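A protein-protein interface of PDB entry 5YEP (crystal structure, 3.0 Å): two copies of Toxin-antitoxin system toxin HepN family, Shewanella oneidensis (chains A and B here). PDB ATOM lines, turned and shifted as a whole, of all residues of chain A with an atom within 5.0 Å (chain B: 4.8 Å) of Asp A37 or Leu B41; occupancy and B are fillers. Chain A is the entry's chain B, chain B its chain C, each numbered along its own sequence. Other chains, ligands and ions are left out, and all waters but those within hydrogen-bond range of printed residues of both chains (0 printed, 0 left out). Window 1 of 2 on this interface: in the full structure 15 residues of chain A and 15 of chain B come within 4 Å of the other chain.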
ATOM      1  N   PHE A  33      20.894  22.722 -26.884  1.00  0.00           N
ATOM      2  CA  PHE A  33      21.724  22.313 -25.754  1.00  0.00           C
ATOM      3  C   PHE A  33      21.330  20.937 -25.234  1.00  0.00           C
ATOM      4  O   PHE A  33      22.180  20.204 -24.717  1.00  0.00           O
ATOM      5  CB  PHE A  33      21.639  23.343 -24.624  1.00  0.00           C
ATOM      6  CG  PHE A  33      22.207  24.690 -24.975  1.00  0.00           C
ATOM      7  CD1 PHE A  33      23.110  24.832 -26.016  1.00  0.00           C
ATOM      8  CD2 PHE A  33      21.835  25.816 -24.260  1.00  0.00           C
ATOM      9  CE1 PHE A  33      23.629  26.072 -26.337  1.00  0.00           C
ATOM     10  CE2 PHE A  33      22.350  27.058 -24.575  1.00  0.00           C
ATOM     11  CZ  PHE A  33      23.249  27.186 -25.615  1.00  0.00           C
ATOM     12  N   THR A  34      20.052  20.567 -25.364  1.00  0.00           N
ATOM     13  CA  THR A  34      19.602  19.270 -24.867  1.00  0.00           C
ATOM     14  C   THR A  34      20.203  18.127 -25.676  1.00  0.00           C
ATOM     15  O   THR A  34      20.588  17.096 -25.112  1.00  0.00           O
ATOM     16  CB  THR A  34      18.074  19.199 -24.887  1.00  0.00           C
ATOM     17  OG1 THR A  34      17.532  20.279 -24.117  1.00  0.00           O
ATOM     18  CG2 THR A  34      17.593  17.880 -24.306  1.00  0.00           C
ATOM     19  N   LEU A  35      20.287  18.287 -26.999  1.00  0.00           N
ATOM     20  CA  LEU A  35      20.973  17.292 -27.815  1.00  0.00           C
ATOM     21  C   LEU A  35      22.449  17.212 -27.447  1.00  0.00           C
ATOM     22  O   LEU A  35      23.046  16.129 -27.465  1.00  0.00           O
ATOM     23  CB  LEU A  35      20.813  17.616 -29.301  1.00  0.00           C
ATOM     24  CG  LEU A  35      19.404  17.659 -29.899  1.00  0.00           C
ATOM     25  CD1 LEU A  35      19.464  18.107 -31.353  1.00  0.00           C
ATOM     26  CD2 LEU A  35      18.697  16.321 -29.774  1.00  0.00           C
ATOM     27  N   GLN A  36      23.052  18.354 -27.110  1.00  0.00           N
ATOM     28  CA  GLN A  36      24.450  18.361 -26.696  1.00  0.00           C
ATOM     29  C   GLN A  36      24.643  17.575 -25.406  1.00  0.00           C
ATOM     30  O   GLN A  36      25.643  16.866 -25.245  1.00  0.00           O
ATOM     31  CB  GLN A  36      24.936  19.801 -26.525  1.00  0.00           C
ATOM     32  CG  GLN A  36      24.746  20.673 -27.755  1.00  0.00           C
ATOM     33  CD  GLN A  36      25.020  22.141 -27.479  1.00  0.00           C
ATOM     34  OE1 GLN A  36      25.685  22.488 -26.503  1.00  0.00           O
ATOM     35  NE2 GLN A  36      24.502  23.012 -28.338  1.00  0.00           N
ATOM     36  N   ASP A  37      23.691  17.684 -24.476  1.00  0.00           N
ATOM     37  CA  ASP A  37      23.805  16.966 -23.212  1.00  0.00           C
ATOM     38  C   ASP A  37      23.634  15.464 -23.409  1.00  0.00           C
ATOM     39  O   ASP A  37      24.345  14.666 -22.787  1.00  0.00           O
ATOM     40  CB  ASP A  37      22.773  17.491 -22.212  1.00  0.00           C
ATOM     41  CG  ASP A  37      22.861  18.995 -22.008  1.00  0.00           C
ATOM     42  OD1 ASP A  37      23.928  19.580 -22.288  1.00  0.00           O
ATOM     43  OD2 ASP A  37      21.858  19.591 -21.562  1.00  0.00           O
ATOM     44  N   SER A  38      22.697  15.059 -24.271  1.00  0.00           N
ATOM     45  CA  SER A  38      22.426  13.640 -24.469  1.00  0.00           C
ATOM     46  C   SER A  38      23.559  12.922 -25.188  1.00  0.00           C
ATOM     47  O   SER A  38      23.658  11.694 -25.094  1.00  0.00           O
ATOM     48  CB  SER A  38      21.122  13.455 -25.246  1.00  0.00           C
ATOM     49  OG  SER A  38      20.902  12.087 -25.542  1.00  0.00           O
ATOM     50  N   VAL A  39      24.406  13.653 -25.907  1.00  0.00           N
ATOM     51  CA  VAL A  39      25.557  13.052 -26.573  1.00  0.00           C
ATOM     52  C   VAL A  39      26.765  13.005 -25.648  1.00  0.00           C
ATOM     53  O   VAL A  39      27.518  12.027 -25.647  1.00  0.00           O
ATOM     54  CB  VAL A  39      25.866  13.822 -27.874  1.00  0.00           C
ATOM     55  CG1 VAL A  39      27.302  13.586 -28.319  1.00  0.00           C
ATOM     56  CG2 VAL A  39      24.893  13.418 -28.971  1.00  0.00           C
ATOM     57  N   ILE A  40      26.955  14.050 -24.839  1.00  0.00           N
ATOM     58  CA  ILE A  40      28.099  14.097 -23.936  1.00  0.00           C
ATOM     59  C   ILE A  40      27.999  13.001 -22.881  1.00  0.00           C
ATOM     60  O   ILE A  40      29.003  12.368 -22.529  1.00  0.00           O
ATOM     61  CB  ILE A  40      28.213  15.496 -23.304  1.00  0.00           C
ATOM     62  CG1 ILE A  40      28.724  16.503 -24.336  1.00  0.00           C
ATOM     63  CG2 ILE A  40      29.122  15.472 -22.085  1.00  0.00           C
ATOM     64  CD1 ILE A  40      28.498  17.946 -23.947  1.00  0.00           C
ATOM     65  N   LEU A  41      26.792  12.746 -22.371  1.00  0.00           N
ATOM     66  CA  LEU A  41      26.626  11.733 -21.333  1.00  0.00           C
ATOM     67  C   LEU A  41      26.942  10.338 -21.861  1.00  0.00           C
ATOM     68  O   LEU A  41      27.645   9.560 -21.206  1.00  0.00           O
ATOM     69  CB  LEU A  41      25.206  11.784 -20.768  1.00  0.00           C
ATOM     70  CG  LEU A  41      24.887  10.714 -19.720  1.00  0.00           C
ATOM     71  CD1 LEU A  41      25.768  10.873 -18.488  1.00  0.00           C
ATOM     72  CD2 LEU A  41      23.418  10.753 -19.339  1.00  0.00           C
ATOM     73  N   ARG B  18      19.167  24.581 -16.081  1.00  0.00           N
ATOM     74  CA  ARG B  18      19.213  23.606 -17.164  1.00  0.00           C
ATOM     75  C   ARG B  18      18.397  22.365 -16.833  1.00  0.00           C
ATOM     76  O   ARG B  18      17.788  21.765 -17.726  1.00  0.00           O
ATOM     77  CB  ARG B  18      20.665  23.229 -17.461  1.00  0.00           C
ATOM     78  CG  ARG B  18      20.867  22.516 -18.783  1.00  0.00           C
ATOM     79  CD  ARG B  18      20.918  23.491 -19.945  1.00  0.00           C
ATOM     80  NE  ARG B  18      20.646  22.813 -21.207  1.00  0.00           N
ATOM     81  CZ  ARG B  18      19.429  22.655 -21.717  1.00  0.00           C
ATOM     82  NH1 ARG B  18      18.372  23.135 -21.077  1.00  0.00           N
ATOM     83  NH2 ARG B  18      19.268  22.019 -22.867  1.00  0.00           N
ATOM     84  N   ASP B  37      18.704  12.050 -20.218  1.00  0.00           N
ATOM     85  CA  ASP B  37      20.158  12.162 -20.269  1.00  0.00           C
ATOM     86  C   ASP B  37      20.620  13.563 -19.896  1.00  0.00           C
ATOM     87  O   ASP B  37      21.660  13.729 -19.248  1.00  0.00           O
ATOM     88  CB  ASP B  37      20.662  11.784 -21.663  1.00  0.00           C
ATOM     89  CG  ASP B  37      20.529  10.297 -21.952  1.00  0.00           C
ATOM     90  OD1 ASP B  37      20.469   9.506 -20.987  1.00  0.00           O
ATOM     91  OD2 ASP B  37      20.485   9.920 -23.144  1.00  0.00           O
ATOM     92  N   SER B  38      19.857  14.586 -20.290  1.00  0.00           N
ATOM     93  CA  SER B  38      20.239  15.960 -19.976  1.00  0.00           C
ATOM     94  C   SER B  38      20.050  16.256 -18.492  1.00  0.00           C
ATOM     95  O   SER B  38      20.913  16.871 -17.856  1.00  0.00           O
ATOM     96  CB  SER B  38      19.430  16.939 -20.829  1.00  0.00           C
ATOM     97  OG  SER B  38      19.798  18.280 -20.558  1.00  0.00           O
ATOM     98  N   VAL B  39      18.917  15.838 -17.926  1.00  0.00           N
ATOM     99  CA  VAL B  39      18.689  16.024 -16.496  1.00  0.00           C
ATOM    100  C   VAL B  39      19.752  15.286 -15.694  1.00  0.00           C
ATOM    101  O   VAL B  39      20.283  15.808 -14.705  1.00  0.00           O
ATOM    102  CB  VAL B  39      17.268  15.565 -16.120  1.00  0.00           C
ATOM    103  CG1 VAL B  39      17.141  15.397 -14.618  1.00  0.00           C
ATOM    104  CG2 VAL B  39      16.242  16.557 -16.635  1.00  0.00           C
ATOM    105  N   ILE B  40      20.094  14.069 -16.120  1.00  0.00           N
ATOM    106  CA  ILE B  40      21.114  13.291 -15.422  1.00  0.00           C
ATOM    107  C   ILE B  40      22.469  13.978 -15.516  1.00  0.00           C
ATOM    108  O   ILE B  40      23.232  14.019 -14.542  1.00  0.00           O
ATOM    109  CB  ILE B  40      21.158  11.858 -15.985  1.00  0.00           C
ATOM    110  CG1 ILE B  40      19.897  11.095 -15.579  1.00  0.00           C
ATOM    111  CG2 ILE B  40      22.399  11.124 -15.502  1.00  0.00           C
ATOM    112  CD1 ILE B  40      19.756   9.758 -16.258  1.00  0.00           C
ATOM    113  N   LEU B  41      22.785  14.545 -16.683  1.00  0.00           N
ATOM    114  CA  LEU B  41      24.093  15.164 -16.875  1.00  0.00           C
ATOM    115  C   LEU B  41      24.260  16.391 -15.988  1.00  0.00           C
ATOM    116  O   LEU B  41      25.294  16.559 -15.332  1.00  0.00           O
ATOM    117  CB  LEU B  41      24.291  15.538 -18.344  1.00  0.00           C
ATOM    118  CG  LEU B  41      25.644  16.178 -18.663  1.00  0.00           C
ATOM    119  CD1 LEU B  41      26.761  15.147 -18.559  1.00  0.00           C
ATOM    120  CD2 LEU B  41      25.633  16.828 -20.035  1.00  0.00           C
ATOM    121  N   ASN B  42      23.249  17.262 -15.954  1.00  0.00           N
ATOM    122  CA  ASN B  42      23.371  18.490 -15.177  1.00  0.00           C
ATOM    123  C   ASN B  42      23.281  18.223 -13.679  1.00  0.00           C
ATOM    124  O   ASN B  42      23.929  18.921 -12.891  1.00  0.00           O
ATOM    125  CB  ASN B  42      22.309  19.494 -15.616  1.00  0.00           C
ATOM    126  CG  ASN B  42      22.458  19.897 -17.070  1.00  0.00           C
ATOM    127  OD1 ASN B  42      23.344  20.676 -17.423  1.00  0.00           O
ATOM    128  ND2 ASN B  42      21.584  19.372 -17.922  1.00  0.00           N
ATOM    129  N   LEU B  43      22.491  17.226 -13.267  1.00  0.00           N
ATOM    130  CA  LEU B  43      22.539  16.779 -11.878  1.00  0.00           C
ATOM    131  C   LEU B  43      23.949  16.355 -11.490  1.00  0.00           C
ATOM    132  O   LEU B  43      24.413  16.646 -10.382  1.00  0.00           O
ATOM    133  CB  LEU B  43      21.562  15.624 -11.657  1.00  0.00           C
ATOM    134  CG  LEU B  43      20.114  15.959 -11.302  1.00  0.00           C
ATOM    135  CD1 LEU B  43      19.319  14.679 -11.119  1.00  0.00           C
ATOM    136  CD2 LEU B  43      20.065  16.799 -10.040  1.00  0.00           C
ATOM    137  N   GLN B  44      24.644  15.665 -12.396  1.00  0.00           N
ATOM    138  CA  GLN B  44      26.029  15.285 -12.142  1.00  0.00           C
ATOM    139  C   GLN B  44      26.938  16.507 -12.099  1.00  0.00           C
ATOM    140  O   GLN B  44      27.861  16.573 -11.279  1.00  0.00           O
ATOM    141  CB  GLN B  44      26.498  14.305 -13.215  1.00  0.00           C
ATOM    142  CG  GLN B  44      27.959  13.916 -13.120  1.00  0.00           C
ATOM    143  CD  GLN B  44      28.406  13.084 -14.300  1.00  0.00           C
ATOM    144  OE1 GLN B  44      27.598  12.719 -15.156  1.00  0.00           O
ATOM    145  NE2 GLN B  44      29.698  12.786 -14.361  1.00  0.00           N
ATOM    146  N   ARG B  45      26.692  17.482 -12.978  1.00  0.00           N
ATOM    147  CA  ARG B  45      27.506  18.694 -12.987  1.00  0.00           C
ATOM    148  C   ARG B  45      27.356  19.471 -11.685  1.00  0.00           C
ATOM    149  O   ARG B  45      28.340  19.999 -11.154  1.00  0.00           O
ATOM    150  CB  ARG B  45      27.131  19.572 -14.182  1.00  0.00           C
ATOM    151  CG  ARG B  45      27.644  19.053 -15.515  1.00  0.00           C
ATOM    152  CD  ARG B  45      27.045  19.820 -16.681  1.00  0.00           C
ATOM    153  NE  ARG B  45      27.773  19.579 -17.923  1.00  0.00           N
ATOM    154  CZ  ARG B  45      27.323  19.908 -19.129  1.00  0.00           C
ATOM    155  NH1 ARG B  45      26.138  20.490 -19.261  1.00  0.00           N
ATOM    156  NH2 ARG B  45      28.055  19.654 -20.205  1.00  0.00           N
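ND2 of Asn B42 lies within hydrogen-bond range of O of Ser B38 (2.6 Å). The side-chain amide oxygen (OD1) of Asn B42 sits at hydrogen-bond distance from the guanidinium group (NH1) of Arg B45, at 3.3 Å.
The side-chain carboxylate of Asp A37 is in salt-bridge range of the guanidinium group of Arg B18. OD2 of Asp B37 lies within hydrogen-bond range of OG of Ser A38 (3.3 Å). The side-chain carboxylate (OD2) of Asp A37 sits at hydrogen-bond distance from the side-chain hydroxyl (OG) of Ser B38 (2.6 Å). The guanidinium group of Arg B18 is in hydrogen-bond range of the side-chain hydroxyl of Thr A34 (2.8 Å). The side-chain carboxylate (OD1) of Asp A37 is in salt-bridge range of the guanidinium group (NH1) of Arg B45 (3.9 Å).
Leu B41 touches just one residue of chain A: Asp A37. Of the printed residues of chain A, Arg B18 touches Phe A33, Thr A34 and Asp A37. Printed residues of chain A within 4 Å of Asn B42: Asp A37 (3.7 Å). Of the printed residues of chain B, Phe A33 touches Arg B18. Ile A40 touches none of the printed residues of chain B. Val B39 touches none of the printed residues of chain A. The nearest residue of chain B that does not touch Asp A37 is Asp B37 (4.5 Å). The nearest residue of chain A that does not touch Leu B41 is Ile A40 (4.3 Å). The nearest printed residue of chain A that does not touch Asp B37 is Asp A37 (4.5 Å).
Among the printed residues, pairs that only touch across the chains: Phe A33 with Arg B18 (3.2 Å), Asp A37 with Leu B41 (3.7 Å), Asp A37 with Asn B42 (3.7 Å), Leu A41 with Asp B37 (3.5 Å) and Leu A41 with Ile B40 (3.99 Å).
Asp A37 touches Ser B38, and with the chains exchanged Ser A38 touches Asp B37. Asp A37 touches Leu B41, and with the chains exchanged Leu A41 touches Asp B37. Leu A41 touches Ile B40, but with the chains exchanged Ile A40 does not touch Leu B41 (4.3 Å). Of the 10 pairs that touch across the chains among the printed residues, 4 have their exchanged pair printed and touching as well.
Of the 10 printed residues of chain B, 7 touch a printed residue of chain A. Hydrophobic or aromatic side chains of chain B that line the printed part of chain A: Ile B40 and Leu B41. Hydrophobic or aromatic side chains of chain A that line the printed part of chain B: Phe A33 and Leu A41. Among the printed residues, 10 pairs touch across the chains.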
